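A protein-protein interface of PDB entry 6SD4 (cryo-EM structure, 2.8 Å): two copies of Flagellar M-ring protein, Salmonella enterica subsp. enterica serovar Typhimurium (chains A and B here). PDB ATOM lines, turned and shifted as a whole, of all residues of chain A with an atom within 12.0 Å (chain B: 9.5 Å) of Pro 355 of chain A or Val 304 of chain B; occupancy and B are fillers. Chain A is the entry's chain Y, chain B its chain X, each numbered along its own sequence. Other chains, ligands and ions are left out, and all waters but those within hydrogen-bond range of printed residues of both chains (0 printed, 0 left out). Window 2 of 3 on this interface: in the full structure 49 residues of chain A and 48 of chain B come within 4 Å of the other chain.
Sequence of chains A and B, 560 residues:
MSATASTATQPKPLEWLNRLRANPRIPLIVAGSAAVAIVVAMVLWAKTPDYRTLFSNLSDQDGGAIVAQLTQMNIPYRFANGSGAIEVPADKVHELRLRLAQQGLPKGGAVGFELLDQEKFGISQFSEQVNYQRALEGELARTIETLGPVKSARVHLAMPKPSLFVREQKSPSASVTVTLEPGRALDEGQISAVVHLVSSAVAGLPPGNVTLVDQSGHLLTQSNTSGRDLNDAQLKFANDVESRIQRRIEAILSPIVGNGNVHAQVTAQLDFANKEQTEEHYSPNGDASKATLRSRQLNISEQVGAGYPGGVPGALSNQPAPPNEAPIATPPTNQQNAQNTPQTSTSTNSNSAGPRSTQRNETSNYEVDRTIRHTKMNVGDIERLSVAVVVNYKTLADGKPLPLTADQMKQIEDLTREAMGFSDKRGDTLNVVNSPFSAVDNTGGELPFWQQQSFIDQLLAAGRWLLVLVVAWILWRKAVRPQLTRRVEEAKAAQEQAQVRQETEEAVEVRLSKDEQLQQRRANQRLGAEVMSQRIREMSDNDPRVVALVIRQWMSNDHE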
ATOM      1  N   SER A 301     -14.100 -12.276  10.659  1.00  0.00           N
ATOM      2  CA  SER A 301     -13.194 -11.544   9.793  1.00  0.00           C
ATOM      3  C   SER A 301     -13.992 -10.605   8.903  1.00  0.00           C
ATOM      4  O   SER A 301     -15.212 -10.725   8.789  1.00  0.00           O
ATOM      5  CB  SER A 301     -12.359 -12.489   8.937  1.00  0.00           C
ATOM      6  OG  SER A 301     -11.561 -11.763   8.027  1.00  0.00           O
ATOM      7  N   GLU A 302     -13.293  -9.662   8.275  1.00  0.00           N
ATOM      8  CA  GLU A 302     -13.940  -8.690   7.396  1.00  0.00           C
ATOM      9  C   GLU A 302     -12.870  -7.800   6.784  1.00  0.00           C
ATOM     10  O   GLU A 302     -12.081  -7.199   7.512  1.00  0.00           O
ATOM     11  CB  GLU A 302     -14.952  -7.856   8.155  1.00  0.00           C
ATOM     12  CG  GLU A 302     -15.403  -6.648   7.393  1.00  0.00           C
ATOM     13  CD  GLU A 302     -16.627  -6.024   8.007  1.00  0.00           C
ATOM     14  OE1 GLU A 302     -16.916  -6.332   9.183  1.00  0.00           O
ATOM     15  OE2 GLU A 302     -17.307  -5.235   7.317  1.00  0.00           O
ATOM     16  N   GLN A 303     -12.855  -7.707   5.463  1.00  0.00           N
ATOM     17  CA  GLN A 303     -11.986  -6.785   4.749  1.00  0.00           C
ATOM     18  C   GLN A 303     -12.849  -5.821   3.955  1.00  0.00           C
ATOM     19  O   GLN A 303     -13.999  -6.132   3.643  1.00  0.00           O
ATOM     20  CB  GLN A 303     -11.034  -7.534   3.823  1.00  0.00           C
ATOM     21  CG  GLN A 303     -10.393  -8.735   4.470  1.00  0.00           C
ATOM     22  CD  GLN A 303      -9.201  -9.235   3.690  1.00  0.00           C
ATOM     23  OE1 GLN A 303      -8.867  -8.696   2.638  1.00  0.00           O
ATOM     24  NE2 GLN A 303      -8.551 -10.270   4.202  1.00  0.00           N
ATOM     25  N   VAL A 304     -12.306  -4.650   3.653  1.00  0.00           N
ATOM     26  CA  VAL A 304     -13.032  -3.651   2.886  1.00  0.00           C
ATOM     27  C   VAL A 304     -12.080  -2.939   1.941  1.00  0.00           C
ATOM     28  O   VAL A 304     -11.110  -3.526   1.465  1.00  0.00           O
ATOM     29  CB  VAL A 304     -13.742  -2.645   3.796  1.00  0.00           C
ATOM     30  CG1 VAL A 304     -14.092  -1.403   3.019  1.00  0.00           C
ATOM     31  CG2 VAL A 304     -14.995  -3.251   4.389  1.00  0.00           C
ATOM     32  N   PRO A 355     -15.128  -4.320  -3.033  1.00  0.00           N
ATOM     33  CA  PRO A 355     -14.388  -5.506  -2.593  1.00  0.00           C
ATOM     34  C   PRO A 355     -14.521  -5.731  -1.090  1.00  0.00           C
ATOM     35  O   PRO A 355     -13.632  -5.369  -0.326  1.00  0.00           O
ATOM     36  CB  PRO A 355     -12.940  -5.185  -2.984  1.00  0.00           C
ATOM     37  CG  PRO A 355     -12.888  -3.707  -3.094  1.00  0.00           C
ATOM     38  CD  PRO A 355     -14.239  -3.266  -3.551  1.00  0.00           C
ATOM     39  N   ARG A 356     -15.625  -6.343  -0.684  1.00  0.00           N
ATOM     40  CA  ARG A 356     -16.016  -6.471   0.717  1.00  0.00           C
ATOM     41  C   ARG A 356     -15.984  -7.950   1.098  1.00  0.00           C
ATOM     42  O   ARG A 356     -17.022  -8.600   1.212  1.00  0.00           O
ATOM     43  CB  ARG A 356     -17.392  -5.863   0.923  1.00  0.00           C
ATOM     44  CG  ARG A 356     -17.854  -5.795   2.353  1.00  0.00           C
ATOM     45  CD  ARG A 356     -18.945  -4.756   2.491  1.00  0.00           C
ATOM     46  NE  ARG A 356     -19.234  -4.429   3.882  1.00  0.00           N
ATOM     47  CZ  ARG A 356     -19.923  -3.360   4.264  1.00  0.00           C
ATOM     48  NH1 ARG A 356     -20.386  -2.513   3.355  1.00  0.00           N
ATOM     49  NH2 ARG A 356     -20.147  -3.134   5.552  1.00  0.00           N
ATOM     50  N   SER A 357     -14.780  -8.474   1.306  1.00  0.00           N
ATOM     51  CA  SER A 357     -14.569  -9.879   1.655  1.00  0.00           C
ATOM     52  C   SER A 357     -14.897 -10.094   3.129  1.00  0.00           C
ATOM     53  O   SER A 357     -14.087  -9.833   4.011  1.00  0.00           O
ATOM     54  CB  SER A 357     -13.138 -10.286   1.338  1.00  0.00           C
ATOM     55  OG  SER A 357     -12.882 -11.618   1.732  1.00  0.00           O
ATOM     56  N   THR A 358     -16.093 -10.602   3.398  1.00  0.00           N
ATOM     57  CA  THR A 358     -16.554 -10.867   4.752  1.00  0.00           C
ATOM     58  C   THR A 358     -16.319 -12.339   5.107  1.00  0.00           C
ATOM     59  O   THR A 358     -15.790 -13.114   4.312  1.00  0.00           O
ATOM     60  CB  THR A 358     -18.029 -10.486   4.870  1.00  0.00           C
ATOM     61  OG1 THR A 358     -18.234  -9.251   4.183  1.00  0.00           O
ATOM     62  CG2 THR A 358     -18.430 -10.265   6.306  1.00  0.00           C
ATOM     63  N   GLN A 359     -16.706 -12.717   6.325  1.00  0.00           N
ATOM     64  CA  GLN A 359     -16.517 -14.062   6.852  1.00  0.00           C
ATOM     65  C   GLN A 359     -17.107 -14.109   8.251  1.00  0.00           C
ATOM     66  O   GLN A 359     -17.204 -13.074   8.907  1.00  0.00           O
ATOM     67  CB  GLN A 359     -15.037 -14.433   6.882  1.00  0.00           C
ATOM     68  CG  GLN A 359     -14.770 -15.886   7.048  1.00  0.00           C
ATOM     69  CD  GLN A 359     -13.476 -16.286   6.392  1.00  0.00           C
ATOM     70  OE1 GLN A 359     -12.848 -15.481   5.706  1.00  0.00           O
ATOM     71  NE2 GLN A 359     -13.067 -17.532   6.591  1.00  0.00           N
ATOM     72  N   SER B 301     -18.762 -17.393   4.823  1.00  0.00           N
ATOM     73  CA  SER B 301     -17.861 -16.565   4.042  1.00  0.00           C
ATOM     74  C   SER B 301     -18.661 -15.769   3.023  1.00  0.00           C
ATOM     75  O   SER B 301     -19.830 -16.058   2.769  1.00  0.00           O
ATOM     76  CB  SER B 301     -16.807 -17.408   3.332  1.00  0.00           C
ATOM     77  OG  SER B 301     -16.007 -16.603   2.495  1.00  0.00           O
ATOM     78  N   GLU B 302     -18.021 -14.756   2.444  1.00  0.00           N
ATOM     79  CA  GLU B 302     -18.678 -13.904   1.454  1.00  0.00           C
ATOM     80  C   GLU B 302     -17.669 -12.893   0.936  1.00  0.00           C
ATOM     81  O   GLU B 302     -17.064 -12.170   1.727  1.00  0.00           O
ATOM     82  CB  GLU B 302     -19.879 -13.198   2.050  1.00  0.00           C
ATOM     83  CG  GLU B 302     -20.389 -12.084   1.189  1.00  0.00           C
ATOM     84  CD  GLU B 302     -21.752 -11.619   1.626  1.00  0.00           C
ATOM     85  OE1 GLU B 302     -22.141 -11.933   2.771  1.00  0.00           O
ATOM     86  OE2 GLU B 302     -22.439 -10.950   0.827  1.00  0.00           O
ATOM     87  N   GLN B 303     -17.502 -12.832  -0.377  1.00  0.00           N
ATOM     88  CA  GLN B 303     -16.683 -11.818  -1.020  1.00  0.00           C
ATOM     89  C   GLN B 303     -17.562 -11.002  -1.950  1.00  0.00           C
ATOM     90  O   GLN B 303     -18.612 -11.477  -2.386  1.00  0.00           O
ATOM     91  CB  GLN B 303     -15.531 -12.452  -1.793  1.00  0.00           C
ATOM     92  CG  GLN B 303     -14.822 -13.536  -1.024  1.00  0.00           C
ATOM     93  CD  GLN B 303     -13.487 -13.887  -1.633  1.00  0.00           C
ATOM     94  OE1 GLN B 303     -13.099 -13.335  -2.661  1.00  0.00           O
ATOM     95  NE2 GLN B 303     -12.772 -14.810  -1.004  1.00  0.00           N
ATOM     96  N   VAL B 304     -17.146  -9.776  -2.235  1.00  0.00           N
ATOM     97  CA  VAL B 304     -17.898  -8.906  -3.126  1.00  0.00           C
ATOM     98  C   VAL B 304     -16.940  -8.094  -3.980  1.00  0.00           C
ATOM     99  O   VAL B 304     -15.850  -8.554  -4.312  1.00  0.00           O
ATOM    100  CB  VAL B 304     -18.844  -7.984  -2.350  1.00  0.00           C
ATOM    101  CG1 VAL B 304     -19.258  -6.822  -3.217  1.00  0.00           C
ATOM    102  CG2 VAL B 304     -20.069  -8.741  -1.887  1.00  0.00           C
ATOM    103  N   PRO B 355     -19.136 -10.009  -9.220  1.00  0.00           N
ATOM    104  CA  PRO B 355     -18.304 -11.071  -8.643  1.00  0.00           C
ATOM    105  C   PRO B 355     -18.591 -11.274  -7.159  1.00  0.00           C
ATOM    106  O   PRO B 355     -17.860 -10.773  -6.311  1.00  0.00           O
ATOM    107  CB  PRO B 355     -16.876 -10.564  -8.873  1.00  0.00           C
ATOM    108  CG  PRO B 355     -17.008  -9.096  -9.039  1.00  0.00           C
ATOM    109  CD  PRO B 355     -18.338  -8.858  -9.671  1.00  0.00           C
ATOM    110  N   ARG B 356     -19.646 -12.021  -6.862  1.00  0.00           N
ATOM    111  CA  ARG B 356     -20.187 -12.165  -5.514  1.00  0.00           C
ATOM    112  C   ARG B 356     -20.005 -13.615  -5.069  1.00  0.00           C
ATOM    113  O   ARG B 356     -20.954 -14.399  -5.053  1.00  0.00           O
ATOM    114  CB  ARG B 356     -21.647 -11.748  -5.499  1.00  0.00           C
ATOM    115  CG  ARG B 356     -22.287 -11.707  -4.140  1.00  0.00           C
ATOM    116  CD  ARG B 356     -23.516 -10.824  -4.177  1.00  0.00           C
ATOM    117  NE  ARG B 356     -24.016 -10.504  -2.845  1.00  0.00           N
ATOM    118  CZ  ARG B 356     -24.884  -9.531  -2.593  1.00  0.00           C
ATOM    119  NH1 ARG B 356     -25.339  -8.781  -3.587  1.00  0.00           N
ATOM    120  NH2 ARG B 356     -25.294  -9.306  -1.353  1.00  0.00           N
ATOM    121  N   SER B 357     -18.778 -13.963  -4.696  1.00  0.00           N
ATOM    122  CA  SER B 357     -18.427 -15.317  -4.266  1.00  0.00           C
ATOM    123  C   SER B 357     -18.903 -15.536  -2.834  1.00  0.00           C
ATOM    124  O   SER B 357     -18.249 -15.145  -1.874  1.00  0.00           O
ATOM    125  CB  SER B 357     -16.924 -15.530  -4.393  1.00  0.00           C
ATOM    126  OG  SER B 357     -16.545 -16.803  -3.914  1.00  0.00           O
ATOM    127  N   THR B 358     -20.043 -16.197  -2.688  1.00  0.00           N
ATOM    128  CA  THR B 358     -20.630 -16.487  -1.389  1.00  0.00           C
ATOM    129  C   THR B 358     -20.246 -17.904  -0.945  1.00  0.00           C
ATOM    130  O   THR B 358     -19.524 -18.619  -1.639  1.00  0.00           O
ATOM    131  CB  THR B 358     -22.145 -16.311  -1.464  1.00  0.00           C
ATOM    132  OG1 THR B 358     -22.427 -15.134  -2.222  1.00  0.00           O
ATOM    133  CG2 THR B 358     -22.748 -16.110  -0.098  1.00  0.00           C
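The backbone carbonyl oxygen of Glu 302 of chain B lies within hydrogen-bond range of the backbone NH of Thr 358 of chain A (2.5 Å).
N of Gln 303 of chain B is in hydrogen-bond range of O of Ser 357 of chain B. The guanidinium group (NH2) of Arg 356 of chain B is in salt-bridge range of the side-chain carboxylate (OE2) of Glu 302 of chain B (3.95 Å). N of Gln 303 of chain A is in hydrogen-bond range of O of Ser 357 of chain A (2.9 Å). OG1 of Thr 358 of chain A sits at hydrogen-bond distance from O of Arg 356 of chain A. OE2 of Glu 302 of chain A is in salt-bridge range of NH2 of Arg 356 of chain A.
Pro 355 of chain A touches Val 304 of chain B. Glu 302 of chain B touches Arg 356 of chain A. CA of Gln 303 of chain B touches O of Arg 356 of chain A, 3.9 Å away. O of Arg 356 of chain A touches N of Val 304 of chain B, at 3.6 Å. Ser 357 of chain A touches Glu 302 of chain B. Gln 303 of chain B touches Ser 357 of chain A. Thr 358 of chain A touches Ser 301 of chain B. CA of Gln 359 of chain A touches CA of Ser 301 of chain B, 3.996 Å away.
Ser 301 of chain A touches none of the printed residues of chain B. Gln 303 of chain A touches none of the printed residues of chain B. No residue of chain B comes within 4 Å of Val 304 of chain A. Pro 355 of chain A touches one residue of chain B. Printed residues of chain B within 4 Å of Arg 356 of chain A: Glu 302, Gln 303 and Val 304. Of the printed residues of chain B, Ser 357 of chain A touches Glu 302 and Gln 303. Of the printed residues of chain B, Thr 358 of chain A touches Ser 301 (3.9 Å) and Glu 302 (2.5 Å). Of the printed residues of chain B, Gln 359 of chain A touches Ser 301 (3.996 Å). Of the printed residues of chain A, Ser 301 of chain B touches Thr 358 and Gln 359. Of chain A, only Arg 356, Ser 357 and Thr 358 come within 4 Å of Glu 302 of chain B. Gln 303 of chain B touches two residues of chain A. Of the printed residues of chain A, Val 304 of chain B touches Pro 355 (3.8 Å) and Arg 356 (3.6 Å). No residue of chain A comes within 4 Å of Pro 355 of chain B. Arg 356 of chain B touches none of the printed residues of chain A. No residue of chain A comes within 4 Å of Ser 357 of chain B. The nearest residue of chain B that does not touch Pro 355 of chain A is Gln 303 of chain B (6.1 Å). The nearest printed residue of chain B that does not touch Ser 357 of chain A is Val 304 of chain B (4.5 Å).
Pro 355 of chain A touches Val 304 of chain B, but with the chains exchanged Val 304 of chain A does not touch Pro 355 of chain B (12.6 Å). Arg 356 of chain A touches Glu 302 of chain B, but with the chains exchanged Glu 302 of chain A does not touch Arg 356 of chain B (12.5 Å). Arg 356 of chain A touches Gln 303 of chain B, but with the chains exchanged Gln 303 of chain A does not touch Arg 356 of chain B (12.6 Å). Thr 358 of chain A touches Ser 301 of chain B, but with the chains exchanged Ser 301 of chain A does not touch Thr 358 of chain B (12.8 Å). Positions printed for both chains: 301, 302, 303, 304, 355, 356, 357 and 358.
Of the 8 printed residues of chain B, 4 touch a printed residue of chain A. Printed residues of chain B that touch a printed residue of chain A: Ser 301, Glu 302, Gln 303 and Val 304. Of the 9 printed residues of chain A, 5 touch a printed residue of chain B. Along chain A the printed residues that touch a printed residue of chain B span positions 355 to 359. Among the printed residues, 9 pairs touch across the chains.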
